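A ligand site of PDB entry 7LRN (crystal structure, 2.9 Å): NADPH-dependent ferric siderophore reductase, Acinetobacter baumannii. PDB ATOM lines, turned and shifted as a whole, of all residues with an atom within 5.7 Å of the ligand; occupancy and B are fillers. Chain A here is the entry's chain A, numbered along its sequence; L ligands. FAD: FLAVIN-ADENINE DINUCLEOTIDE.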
ATOM      1  N   ALA A  78      17.721 -29.500  20.841  1.00  0.00           N
ATOM      2  CA  ALA A  78      18.810 -29.285  21.762  1.00  0.00           C
ATOM      3  C   ALA A  78      19.439 -30.628  22.127  1.00  0.00           C
ATOM      4  O   ALA A  78      18.811 -31.683  22.027  1.00  0.00           O
ATOM      5  CB  ALA A  78      18.345 -28.532  23.002  1.00  0.00           C
ATOM      6  N   ARG A  94      25.621 -30.469  29.895  1.00  0.00           N
ATOM      7  CA  ARG A  94      25.031 -29.165  29.700  1.00  0.00           C
ATOM      8  C   ARG A  94      24.228 -29.179  28.410  1.00  0.00           C
ATOM      9  O   ARG A  94      24.548 -29.930  27.491  1.00  0.00           O
ATOM     10  CB  ARG A  94      26.112 -28.095  29.672  1.00  0.00           C
ATOM     11  CG  ARG A  94      26.852 -27.906  30.970  1.00  0.00           C
ATOM     12  CD  ARG A  94      26.061 -27.081  31.927  1.00  0.00           C
ATOM     13  NE  ARG A  94      26.680 -27.008  33.243  1.00  0.00           N
ATOM     14  CZ  ARG A  94      26.438 -27.839  34.252  1.00  0.00           C
ATOM     15  NH1 ARG A  94      25.572 -28.846  34.130  1.00  0.00           N
ATOM     16  NH2 ARG A  94      27.057 -27.654  35.403  1.00  0.00           N
ATOM     17  N   VAL A  95      23.189 -28.352  28.343  1.00  0.00           N
ATOM     18  CA  VAL A  95      22.244 -28.333  27.222  1.00  0.00           C
ATOM     19  C   VAL A  95      22.590 -27.161  26.289  1.00  0.00           C
ATOM     20  O   VAL A  95      22.659 -26.006  26.732  1.00  0.00           O
ATOM     21  CB  VAL A  95      20.787 -28.246  27.739  1.00  0.00           C
ATOM     22  CG1 VAL A  95      19.782 -28.203  26.617  1.00  0.00           C
ATOM     23  CG2 VAL A  95      20.467 -29.450  28.659  1.00  0.00           C
ATOM     24  N   TYR A  96      22.770 -27.450  24.990  1.00  0.00           N
ATOM     25  CA  TYR A  96      23.060 -26.459  23.963  1.00  0.00           C
ATOM     26  C   TYR A  96      22.189 -26.716  22.733  1.00  0.00           C
ATOM     27  O   TYR A  96      21.776 -27.844  22.478  1.00  0.00           O
ATOM     28  CB  TYR A  96      24.543 -26.468  23.576  1.00  0.00           C
ATOM     29  CG  TYR A  96      25.382 -25.776  24.605  1.00  0.00           C
ATOM     30  CD1 TYR A  96      25.643 -24.414  24.497  1.00  0.00           C
ATOM     31  CD2 TYR A  96      25.844 -26.448  25.743  1.00  0.00           C
ATOM     32  CE1 TYR A  96      26.364 -23.734  25.464  1.00  0.00           C
ATOM     33  CE2 TYR A  96      26.582 -25.757  26.735  1.00  0.00           C
ATOM     34  CZ  TYR A  96      26.834 -24.385  26.572  1.00  0.00           C
ATOM     35  OH  TYR A  96      27.548 -23.645  27.488  1.00  0.00           O
ATOM     36  N   THR A  97      21.886 -25.665  21.981  1.00  0.00           N
ATOM     37  CA  THR A  97      21.020 -25.814  20.826  1.00  0.00           C
ATOM     38  C   THR A  97      21.799 -26.266  19.594  1.00  0.00           C
ATOM     39  O   THR A  97      22.960 -25.858  19.403  1.00  0.00           O
ATOM     40  CB  THR A  97      20.304 -24.506  20.527  1.00  0.00           C
ATOM     41  OG1 THR A  97      19.688 -24.018  21.724  1.00  0.00           O
ATOM     42  CG2 THR A  97      19.242 -24.704  19.457  1.00  0.00           C
ATOM     43  N   VAL A  98      21.186 -27.109  18.764  1.00  0.00           N
ATOM     44  CA  VAL A  98      21.759 -27.441  17.454  1.00  0.00           C
ATOM     45  C   VAL A  98      21.442 -26.262  16.524  1.00  0.00           C
ATOM     46  O   VAL A  98      20.305 -26.072  16.092  1.00  0.00           O
ATOM     47  CB  VAL A  98      21.226 -28.773  16.896  1.00  0.00           C
ATOM     48  CG1 VAL A  98      21.534 -29.919  17.838  1.00  0.00           C
ATOM     49  CG2 VAL A  98      19.732 -28.731  16.652  1.00  0.00           C
ATOM     50  N   ILE A 110      27.007 -25.548  17.053  1.00  0.00           N
ATOM     51  CA  ILE A 110      26.588 -25.065  18.363  1.00  0.00           C
ATOM     52  C   ILE A 110      27.255 -23.725  18.649  1.00  0.00           C
ATOM     53  O   ILE A 110      28.476 -23.577  18.479  1.00  0.00           O
ATOM     54  CB  ILE A 110      26.924 -26.070  19.481  1.00  0.00           C
ATOM     55  CG1 ILE A 110      26.235 -27.415  19.211  1.00  0.00           C
ATOM     56  CG2 ILE A 110      26.563 -25.452  20.826  1.00  0.00           C
ATOM     57  CD1 ILE A 110      26.868 -28.594  19.916  1.00  0.00           C
ATOM     58  N   ASP A 111      26.467 -22.757  19.108  1.00  0.00           N
ATOM     59  CA  ASP A 111      26.980 -21.485  19.597  1.00  0.00           C
ATOM     60  C   ASP A 111      27.074 -21.491  21.116  1.00  0.00           C
ATOM     61  O   ASP A 111      26.094 -21.774  21.808  1.00  0.00           O
ATOM     62  CB  ASP A 111      26.058 -20.339  19.145  1.00  0.00           C
ATOM     63  CG  ASP A 111      26.245 -19.976  17.668  1.00  0.00           C
ATOM     64  OD1 ASP A 111      27.223 -20.451  17.032  1.00  0.00           O
ATOM     65  OD2 ASP A 111      25.359 -19.235  17.159  1.00  0.00           O
ATOM     66  N   PHE A 112      28.247 -21.174  21.635  1.00  0.00           N
ATOM     67  CA  PHE A 112      28.426 -21.063  23.076  1.00  0.00           C
ATOM     68  C   PHE A 112      28.510 -19.593  23.470  1.00  0.00           C
ATOM     69  O   PHE A 112      29.323 -18.843  22.933  1.00  0.00           O
ATOM     70  CB  PHE A 112      29.679 -21.785  23.538  1.00  0.00           C
ATOM     71  CG  PHE A 112      29.641 -23.244  23.326  1.00  0.00           C
ATOM     72  CD1 PHE A 112      29.684 -23.781  22.053  1.00  0.00           C
ATOM     73  CD2 PHE A 112      29.561 -24.097  24.410  1.00  0.00           C
ATOM     74  CE1 PHE A 112      29.658 -25.169  21.854  1.00  0.00           C
ATOM     75  CE2 PHE A 112      29.540 -25.473  24.222  1.00  0.00           C
ATOM     76  CZ  PHE A 112      29.577 -26.009  22.940  1.00  0.00           C
ATOM     77  N   VAL A 113      27.653 -19.174  24.401  1.00  0.00           N
ATOM     78  CA  VAL A 113      27.752 -17.847  24.971  1.00  0.00           C
ATOM     79  C   VAL A 113      28.895 -17.863  25.986  1.00  0.00           C
ATOM     80  O   VAL A 113      28.829 -18.601  26.970  1.00  0.00           O
ATOM     81  CB  VAL A 113      26.436 -17.420  25.626  1.00  0.00           C
ATOM     82  CG1 VAL A 113      26.657 -16.189  26.407  1.00  0.00           C
ATOM     83  CG2 VAL A 113      25.336 -17.193  24.591  1.00  0.00           C
ATOM     84  N   LYS A 114      29.931 -17.085  25.737  1.00  0.00           N
ATOM     85  CA  LYS A 114      30.990 -16.951  26.723  1.00  0.00           C
ATOM     86  C   LYS A 114      30.458 -16.183  27.928  1.00  0.00           C
ATOM     87  O   LYS A 114      29.731 -15.195  27.775  1.00  0.00           O
ATOM     88  CB  LYS A 114      32.200 -16.186  26.141  1.00  0.00           C
ATOM     89  CG  LYS A 114      32.986 -16.902  25.035  1.00  0.00           C
ATOM     90  CD  LYS A 114      33.905 -15.902  24.241  1.00  0.00           C
ATOM     91  CE  LYS A 114      35.220 -15.586  24.969  1.00  0.00           C
ATOM     92  NZ  LYS A 114      35.971 -16.821  25.431  1.00  0.00           N
ATOM     93  N   HIS A 115      30.814 -16.624  29.130  1.00  0.00           N
ATOM     94  CA  HIS A 115      30.442 -15.891  30.332  1.00  0.00           C
ATOM     95  C   HIS A 115      31.498 -16.123  31.413  1.00  0.00           C
ATOM     96  O   HIS A 115      32.027 -17.232  31.542  1.00  0.00           O
ATOM     97  CB  HIS A 115      29.010 -16.275  30.793  1.00  0.00           C
ATOM     98  CG  HIS A 115      28.811 -17.737  31.031  1.00  0.00           C
ATOM     99  ND1 HIS A 115      28.931 -18.311  32.287  1.00  0.00           N
ATOM    100  CD2 HIS A 115      28.485 -18.742  30.196  1.00  0.00           C
ATOM    101  CE1 HIS A 115      28.709 -19.607  32.193  1.00  0.00           C
ATOM    102  NE2 HIS A 115      28.433 -19.900  30.935  1.00  0.00           N
ATOM    103  N   ASP A 117      32.750 -17.231  34.204  1.00  0.00           N
ATOM    104  CA  ASP A 117      32.350 -18.226  35.204  1.00  0.00           C
ATOM    105  C   ASP A 117      33.283 -19.422  35.075  1.00  0.00           C
ATOM    106  O   ASP A 117      33.457 -19.931  33.970  1.00  0.00           O
ATOM    107  CB  ASP A 117      30.928 -18.746  34.971  1.00  0.00           C
ATOM    108  CG  ASP A 117      29.861 -17.821  35.492  1.00  0.00           C
ATOM    109  OD1 ASP A 117      29.756 -17.668  36.740  1.00  0.00           O
ATOM    110  OD2 ASP A 117      29.103 -17.271  34.651  1.00  0.00           O
ATOM    111  N   SER A 119      32.717 -22.365  35.104  1.00  0.00           N
ATOM    112  CA  SER A 119      31.714 -23.403  34.971  1.00  0.00           C
ATOM    113  C   SER A 119      32.257 -24.567  34.154  1.00  0.00           C
ATOM    114  O   SER A 119      33.292 -24.426  33.502  1.00  0.00           O
ATOM    115  CB  SER A 119      30.479 -22.845  34.280  1.00  0.00           C
ATOM    116  OG  SER A 119      30.740 -22.675  32.898  1.00  0.00           O
ATOM    117  N   PRO A 120      31.586 -25.738  34.177  1.00  0.00           N
ATOM    118  CA  PRO A 120      31.993 -26.829  33.299  1.00  0.00           C
ATOM    119  C   PRO A 120      32.049 -26.499  31.819  1.00  0.00           C
ATOM    120  O   PRO A 120      33.084 -26.716  31.184  1.00  0.00           O
ATOM    121  CB  PRO A 120      30.927 -27.897  33.572  1.00  0.00           C
ATOM    122  CG  PRO A 120      30.603 -27.706  34.974  1.00  0.00           C
ATOM    123  CD  PRO A 120      30.674 -26.216  35.227  1.00  0.00           C
ATOM    124  N   ALA A 121      30.968 -25.984  31.231  1.00  0.00           N
ATOM    125  CA  ALA A 121      31.004 -25.723  29.797  1.00  0.00           C
ATOM    126  C   ALA A 121      32.070 -24.692  29.454  1.00  0.00           C
ATOM    127  O   ALA A 121      32.701 -24.788  28.399  1.00  0.00           O
ATOM    128  CB  ALA A 121      29.626 -25.298  29.279  1.00  0.00           C
ATOM    129  N   MET A 122      32.303 -23.726  30.333  1.00  0.00           N
ATOM    130  CA  MET A 122      33.342 -22.736  30.071  1.00  0.00           C
ATOM    131  C   MET A 122      34.744 -23.338  30.186  1.00  0.00           C
ATOM    132  O   MET A 122      35.625 -23.053  29.366  1.00  0.00           O
ATOM    133  CB  MET A 122      33.148 -21.544  31.011  1.00  0.00           C
ATOM    134  CG  MET A 122      31.952 -20.664  30.613  1.00  0.00           C
ATOM    135  SD  MET A 122      31.928 -20.217  28.840  1.00  0.00           S
ATOM    136  CE  MET A 122      30.582 -21.222  28.175  1.00  0.00           C
ATOM    137  N   HIS A 142      12.277 -28.912  21.092  1.00  0.00           N
ATOM    138  CA  HIS A 142      11.916 -27.855  22.019  1.00  0.00           C
ATOM    139  C   HIS A 142      10.891 -26.924  21.364  1.00  0.00           C
ATOM    140  O   HIS A 142      10.547 -27.074  20.192  1.00  0.00           O
ATOM    141  CB  HIS A 142      13.150 -27.095  22.484  1.00  0.00           C
ATOM    142  CG  HIS A 142      13.764 -27.679  23.718  1.00  0.00           C
ATOM    143  ND1 HIS A 142      13.629 -27.099  24.956  1.00  0.00           N
ATOM    144  CD2 HIS A 142      14.494 -28.803  23.903  1.00  0.00           C
ATOM    145  CE1 HIS A 142      14.268 -27.838  25.854  1.00  0.00           C
ATOM    146  NE2 HIS A 142      14.802 -28.878  25.241  1.00  0.00           N
ATOM    147  N   ASP A 159      20.985 -14.073  24.674  1.00  0.00           N
ATOM    148  CA  ASP A 159      22.095 -14.643  23.920  1.00  0.00           C
ATOM    149  C   ASP A 159      22.034 -16.161  23.848  1.00  0.00           C
ATOM    150  O   ASP A 159      22.488 -16.757  22.869  1.00  0.00           O
ATOM    151  CB  ASP A 159      23.426 -14.175  24.515  1.00  0.00           C
ATOM    152  CG  ASP A 159      23.966 -12.939  23.821  1.00  0.00           C
ATOM    153  OD1 ASP A 159      23.710 -12.819  22.601  1.00  0.00           O
ATOM    154  OD2 ASP A 159      24.662 -12.124  24.465  1.00  0.00           O
ATOM    155  N   THR A 160      21.474 -16.812  24.866  1.00  0.00           N
ATOM    156  CA  THR A 160      21.445 -18.267  24.892  1.00  0.00           C
ATOM    157  C   THR A 160      20.418 -18.846  23.937  1.00  0.00           C
ATOM    158  O   THR A 160      20.536 -20.005  23.525  1.00  0.00           O
ATOM    159  CB  THR A 160      21.180 -18.748  26.313  1.00  0.00           C
ATOM    160  OG1 THR A 160      19.902 -18.265  26.738  1.00  0.00           O
ATOM    161  CG2 THR A 160      22.276 -18.231  27.280  1.00  0.00           C
ATOM    162  N   ALA A 161      19.419 -18.077  23.561  1.00  0.00           N
ATOM    163  CA  ALA A 161      18.370 -18.565  22.689  1.00  0.00           C
ATOM    164  C   ALA A 161      18.506 -18.067  21.270  1.00  0.00           C
ATOM    165  O   ALA A 161      17.642 -18.351  20.431  1.00  0.00           O
ATOM    166  CB  ALA A 161      17.009 -18.176  23.259  1.00  0.00           C
ATOM    167  N   PRO A 163      20.768 -19.143  19.031  1.00  0.00           N
ATOM    168  CA  PRO A 163      20.792 -20.352  18.173  1.00  0.00           C
ATOM    169  C   PRO A 163      19.422 -20.984  17.949  1.00  0.00           C
ATOM    170  O   PRO A 163      19.096 -21.319  16.802  1.00  0.00           O
ATOM    171  CB  PRO A 163      21.756 -21.277  18.916  1.00  0.00           C
ATOM    172  CG  PRO A 163      22.639 -20.366  19.668  1.00  0.00           C
ATOM    173  CD  PRO A 163      21.759 -19.238  20.118  1.00  0.00           C
ATOM    174  N   ALA A 164      18.617 -21.186  19.001  1.00  0.00           N
ATOM    175  CA  ALA A 164      17.245 -21.677  18.796  1.00  0.00           C
ATOM    176  C   ALA A 164      16.457 -20.809  17.802  1.00  0.00           C
ATOM    177  O   ALA A 164      15.685 -21.322  16.988  1.00  0.00           O
ATOM    178  CB  ALA A 164      16.511 -21.772  20.140  1.00  0.00           C
ATOM    179  N   GLY A 262      12.962 -21.043  30.134  1.00  0.00           N
ATOM    180  CA  GLY A 262      14.104 -20.417  30.757  1.00  0.00           C
ATOM    181  C   GLY A 262      15.329 -21.253  30.482  1.00  0.00           C
ATOM    182  O   GLY A 262      15.454 -22.357  31.022  1.00  0.00           O
ATOM    183  N   TYR A 263      16.229 -20.773  29.596  1.00  0.00           N
ATOM    184  CA  TYR A 263      17.402 -21.551  29.189  1.00  0.00           C
ATOM    185  C   TYR A 263      18.449 -21.614  30.288  1.00  0.00           C
ATOM    186  O   TYR A 263      19.232 -22.571  30.310  1.00  0.00           O
ATOM    187  CB  TYR A 263      17.995 -20.993  27.889  1.00  0.00           C
ATOM    188  CG  TYR A 263      17.261 -21.477  26.625  1.00  0.00           C
ATOM    189  CD1 TYR A 263      16.092 -22.192  26.756  1.00  0.00           C
ATOM    190  CD2 TYR A 263      17.751 -21.233  25.328  1.00  0.00           C
ATOM    191  CE1 TYR A 263      15.404 -22.656  25.663  1.00  0.00           C
ATOM    192  CE2 TYR A 263      17.051 -21.713  24.203  1.00  0.00           C
ATOM    193  CZ  TYR A 263      15.867 -22.416  24.413  1.00  0.00           C
ATOM    194  OH  TYR A 263      15.075 -22.926  23.396  1.00  0.00           O
ATOM    195  N   TRP A 264      18.459 -20.665  31.227  1.00  0.00           N
ATOM    196  CA  TRP A 264      19.440 -20.663  32.296  1.00  0.00           C
ATOM    197  C   TRP A 264      18.931 -19.794  33.444  1.00  0.00           C
ATOM    198  O   TRP A 264      17.946 -19.076  33.295  1.00  0.00           O
ATOM    199  CB  TRP A 264      20.787 -20.147  31.790  1.00  0.00           C
ATOM    200  CG  TRP A 264      20.740 -18.726  31.358  1.00  0.00           C
ATOM    201  CD1 TRP A 264      20.137 -18.220  30.233  1.00  0.00           C
ATOM    202  CD2 TRP A 264      21.309 -17.604  32.040  1.00  0.00           C
ATOM    203  NE1 TRP A 264      20.308 -16.857  30.185  1.00  0.00           N
ATOM    204  CE2 TRP A 264      21.026 -16.457  31.285  1.00  0.00           C
ATOM    205  CE3 TRP A 264      22.039 -17.468  33.237  1.00  0.00           C
ATOM    206  CZ2 TRP A 264      21.443 -15.202  31.668  1.00  0.00           C
ATOM    207  CZ3 TRP A 264      22.440 -16.233  33.605  1.00  0.00           C
ATOM    208  CH2 TRP A 264      22.152 -15.103  32.826  1.00  0.00           C
ATOM    209  N   ARG A 265      19.622 -19.829  34.573  1.00  0.00           N
ATOM    210  CA  ARG A 265      19.157 -19.099  35.746  1.00  0.00           C
ATOM    211  C   ARG A 265      20.325 -18.494  36.526  1.00  0.00           C
ATOM    212  O   ARG A 265      21.233 -19.207  36.943  1.00  0.00           O
ATOM    213  CB  ARG A 265      18.352 -20.031  36.652  1.00  0.00           C
ATOM    214  CG  ARG A 265      17.959 -19.394  37.961  1.00  0.00           C
ATOM    215  CD  ARG A 265      16.852 -20.117  38.633  1.00  0.00           C
ATOM    216  NE  ARG A 265      16.607 -19.618  39.973  1.00  0.00           N
ATOM    217  CZ  ARG A 265      15.682 -20.127  40.772  1.00  0.00           C
ATOM    218  NH1 ARG A 265      14.895 -21.107  40.372  1.00  0.00           N
ATOM    219  NH2 ARG A 265      15.558 -19.662  42.012  1.00  0.00           N
ATOM    220  N   ASP A 266      20.257 -17.185  36.790  1.00  0.00           N
ATOM    221  CA  ASP A 266      21.414 -16.493  37.346  1.00  0.00           C
ATOM    222  C   ASP A 266      21.642 -16.894  38.796  1.00  0.00           C
ATOM    223  O   ASP A 266      20.744 -16.758  39.645  1.00  0.00           O
ATOM    224  CB  ASP A 266      21.215 -14.986  37.252  1.00  0.00           C
ATOM    225  CG  ASP A 266      22.534 -14.209  37.420  1.00  0.00           C
ATOM    226  OD1 ASP A 266      23.592 -14.848  37.676  1.00  0.00           O
ATOM    227  OD2 ASP A 266      22.509 -12.968  37.280  1.00  0.00           O
ATOM    228  N   GLY A 267      22.864 -17.361  39.098  1.00  0.00           N
ATOM    229  CA  GLY A 267      23.215 -17.833  40.415  1.00  0.00           C
ATOM    230  C   GLY A 267      22.982 -19.312  40.652  1.00  0.00           C
ATOM    231  O   GLY A 267      23.317 -19.831  41.731  1.00  0.00           O
ATOM    232  N   VAL A 268      22.356 -20.008  39.697  1.00  0.00           N
ATOM    233  CA  VAL A 268      22.072 -21.425  39.816  1.00  0.00           C
ATOM    234  C   VAL A 268      22.744 -22.135  38.635  1.00  0.00           C
ATOM    235  O   VAL A 268      22.745 -21.622  37.519  1.00  0.00           O
ATOM    236  CB  VAL A 268      20.548 -21.690  39.827  1.00  0.00           C
ATOM    237  CG1 VAL A 268      20.245 -23.094  40.232  1.00  0.00           C
ATOM    238  CG2 VAL A 268      19.872 -20.726  40.787  1.00  0.00           C
ATOM    239  N   SER A 269      23.363 -23.286  38.904  1.00  0.00           N
ATOM    240  CA  SER A 269      24.010 -23.997  37.820  1.00  0.00           C
ATOM    241  C   SER A 269      22.989 -24.889  37.130  1.00  0.00           C
ATOM    242  O   SER A 269      21.952 -25.230  37.693  1.00  0.00           O
ATOM    243  CB  SER A 269      25.189 -24.846  38.312  1.00  0.00           C
ATOM    244  OG  SER A 269      24.809 -26.086  38.917  1.00  0.00           O
ATOM    245  N   SER A 270      23.294 -25.248  35.876  1.00  0.00           N
ATOM    246  CA  SER A 270      22.451 -26.197  35.151  1.00  0.00           C
ATOM    247  C   SER A 270      22.202 -27.459  35.956  1.00  0.00           C
ATOM    248  O   SER A 270      21.073 -27.958  36.007  1.00  0.00           O
ATOM    249  CB  SER A 270      23.108 -26.561  33.822  1.00  0.00           C
ATOM    250  OG  SER A 270      22.470 -27.703  33.281  1.00  0.00           O
ATOM    251  N   SER A 271      23.231 -28.005  36.607  1.00  0.00           N
ATOM    252  CA  SER A 271      23.044 -29.196  37.410  1.00  0.00           C
ATOM    253  C   SER A 271      21.980 -28.982  38.480  1.00  0.00           C
ATOM    254  O   SER A 271      21.118 -29.839  38.695  1.00  0.00           O
ATOM    255  CB  SER A 271      24.369 -29.615  38.061  1.00  0.00           C
ATOM    256  OG  SER A 271      25.385 -29.880  37.114  1.00  0.00           O
HETATM  257  PA  FAD L   1      26.730 -23.578  34.897  1.00  0.00           P
HETATM  258  O1A FAD L   1      27.771 -24.435  35.691  1.00  0.00           O
HETATM  259  O2A FAD L   1      25.383 -24.088  34.683  1.00  0.00           O
HETATM  260  O5B FAD L   1      26.482 -22.220  35.414  1.00  0.00           O
HETATM  261  C5B FAD L   1      27.022 -21.794  36.632  1.00  0.00           C
HETATM  262  C4B FAD L   1      26.890 -20.271  36.666  1.00  0.00           C
HETATM  263  O4B FAD L   1      26.996 -19.703  35.396  1.00  0.00           O
HETATM  264  C3B FAD L   1      25.550 -19.935  37.225  1.00  0.00           C
HETATM  265  O3B FAD L   1      25.609 -18.949  38.181  1.00  0.00           O
HETATM  266  C2B FAD L   1      24.775 -19.465  36.053  1.00  0.00           C
HETATM  267  O2B FAD L   1      23.846 -18.518  36.416  1.00  0.00           O
HETATM  268  C1B FAD L   1      25.849 -18.899  35.181  1.00  0.00           C
HETATM  269  N9A FAD L   1      25.567 -18.893  33.761  1.00  0.00           N
HETATM  270  C8A FAD L   1      25.274 -19.980  32.954  1.00  0.00           C
HETATM  271  N7A FAD L   1      25.083 -19.585  31.692  1.00  0.00           N
HETATM  272  C5A FAD L   1      25.232 -18.196  31.613  1.00  0.00           C
HETATM  273  C6A FAD L   1      25.139 -17.272  30.574  1.00  0.00           C
HETATM  274  N6A FAD L   1      24.834 -17.670  29.210  1.00  0.00           N
HETATM  275  N1A FAD L   1      25.327 -15.965  30.852  1.00  0.00           N
HETATM  276  C2A FAD L   1      25.609 -15.550  32.120  1.00  0.00           C
HETATM  277  N3A FAD L   1      25.732 -16.424  33.143  1.00  0.00           N
HETATM  278  C4A FAD L   1      25.559 -17.743  32.928  1.00  0.00           C
HETATM  279  N1  FAD L   1      23.629 -21.682  25.983  1.00  0.00           N
HETATM  280  C2  FAD L   1      24.458 -21.271  24.874  1.00  0.00           C
HETATM  281  O2  FAD L   1      25.586 -20.530  25.100  1.00  0.00           O
HETATM  282  N3  FAD L   1      24.130 -21.642  23.583  1.00  0.00           N
HETATM  283  C4  FAD L   1      22.985 -22.390  23.345  1.00  0.00           C
HETATM  284  O4  FAD L   1      22.577 -22.815  22.110  1.00  0.00           O
HETATM  285  C4X FAD L   1      22.127 -22.809  24.449  1.00  0.00           C
HETATM  286  N5  FAD L   1      21.021 -23.563  24.153  1.00  0.00           N
HETATM  287  C5X FAD L   1      20.212 -23.977  25.181  1.00  0.00           C
HETATM  288  C6  FAD L   1      19.100 -24.744  24.836  1.00  0.00           C
HETATM  289  C7  FAD L   1      18.262 -25.162  25.873  1.00  0.00           C
HETATM  290  C7M FAD L   1      17.061 -25.973  25.529  1.00  0.00           C
HETATM  291  C8  FAD L   1      18.533 -24.845  27.190  1.00  0.00           C
HETATM  292  C8M FAD L   1      17.609 -25.326  28.249  1.00  0.00           C
HETATM  293  C9  FAD L   1      19.665 -24.099  27.542  1.00  0.00           C
HETATM  294  C9A FAD L   1      20.501 -23.663  26.521  1.00  0.00           C
HETATM  295  N10 FAD L   1      21.652 -22.884  26.824  1.00  0.00           N
HETATM  296  C10 FAD L   1      22.492 -22.444  25.787  1.00  0.00           C
HETATM  297  C1' FAD L   1      21.943 -22.516  28.221  1.00  0.00           C
HETATM  298  C2' FAD L   1      23.076 -23.330  28.805  1.00  0.00           C
HETATM  299  O2' FAD L   1      22.670 -24.626  28.921  1.00  0.00           O
HETATM  300  C3' FAD L   1      23.423 -22.704  30.166  1.00  0.00           C
HETATM  301  O3' FAD L   1      23.789 -21.392  29.955  1.00  0.00           O
HETATM  302  C4' FAD L   1      24.464 -23.429  30.989  1.00  0.00           C
HETATM  303  O4' FAD L   1      24.148 -23.176  32.302  1.00  0.00           O
HETATM  304  C5' FAD L   1      25.890 -23.011  30.756  1.00  0.00           C
HETATM  305  O5' FAD L   1      26.763 -24.027  31.187  1.00  0.00           O
HETATM  306  P   FAD L   1      27.843 -23.851  32.368  1.00  0.00           P
HETATM  307  O1P FAD L   1      28.748 -25.085  32.783  1.00  0.00           O
HETATM  308  O2P FAD L   1      28.508 -22.527  31.830  1.00  0.00           O
HETATM  309  O3P FAD L   1      26.906 -23.123  33.493  1.00  0.00           O
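The side-chain hydroxyl of Ser 119 lies within hydrogen-bond range of an oxygen (O2P) of the ligand. N of Val 113 lies within hydrogen-bond range of O2 of the ligand. O of Val 95 lies within hydrogen-bond range of O2' of the ligand (2.6 Å). The backbone carbonyl oxygen (O) of Asp 111 is in hydrogen-bond range of a nitrogen (N3) of the ligand, at 2.7 Å. An oxygen (O2A) of the ligand is in hydrogen-bond range of the backbone NH of Ser 270, at 2.7 Å. The backbone carbonyl oxygen (O) of Arg 265 is in hydrogen-bond range of an oxygen (O2B) of the ligand (2.8 Å). NE2 of His 115 is in hydrogen-bond range of O2P of the ligand, 2.8 Å away. N of Thr 97 sits at hydrogen-bond distance from O4 of the ligand (2.9 Å). A nitrogen (N5) of the ligand is in hydrogen-bond range of the side-chain hydroxyl (OG1) of Thr 97, at 2.8 Å. N of Ala 121 is in hydrogen-bond range of O1P of the ligand (2.9 Å). NE of Arg 94 is in salt-bridge range of O1P of the ligand (2.9 Å). An oxygen (O2B) of the ligand lies within hydrogen-bond range of the backbone NH (N) of Gly 267, at 3.1 Å. O2B of the ligand sits close to O of Val 268, 3.5 Å away.
OG of Ser 119 lies within hydrogen-bond range of N of Met 122, 3.2 Å away. OG of Ser 270 lies close to NH1 of Arg 94, 3.4 Å away. A ring nitrogen (ND1) of His 115 lies within hydrogen-bond range of the side-chain carboxylate (OD2) of Asp 117, 2.6 Å away. N of His 115 sits at hydrogen-bond distance from SD of Met 122 (3.8 Å). OG of Ser 271 lies within hydrogen-bond range of NH1 of Arg 94 (3.2 Å). The backbone NH (N) of Ser 271 sits close to the side-chain hydroxyl (OG) of Ser 269 (3.4 Å).
The side-chain carboxylate (OD2) of Asp 117 lies close to an oxygen (O4B) of the ligand (3.3 Å). The backbone nitrogen of Pro 120 sits close to an oxygen (O1P) of the ligand (3.2 Å). CB of Ala 78 touches C7M of the ligand (3.8 Å). Tyr 96 touches the ligand. C of Phe 112 touches O2 of the ligand, at 3.5 Å. His 142 touches the ligand. CG2 of Thr 160 touches N6A of the ligand, at 3.3 Å. Pro 163 touches the ligand. O of Tyr 263 touches C9 of the ligand, at 3.2 Å. Trp 264 touches the ligand (CZ3 to N3A, 3.3 Å). CA of Asp 266 touches O2B of the ligand, 3.3 Å away. Ser 269 touches the ligand (CA to O2A, 3.4 Å).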
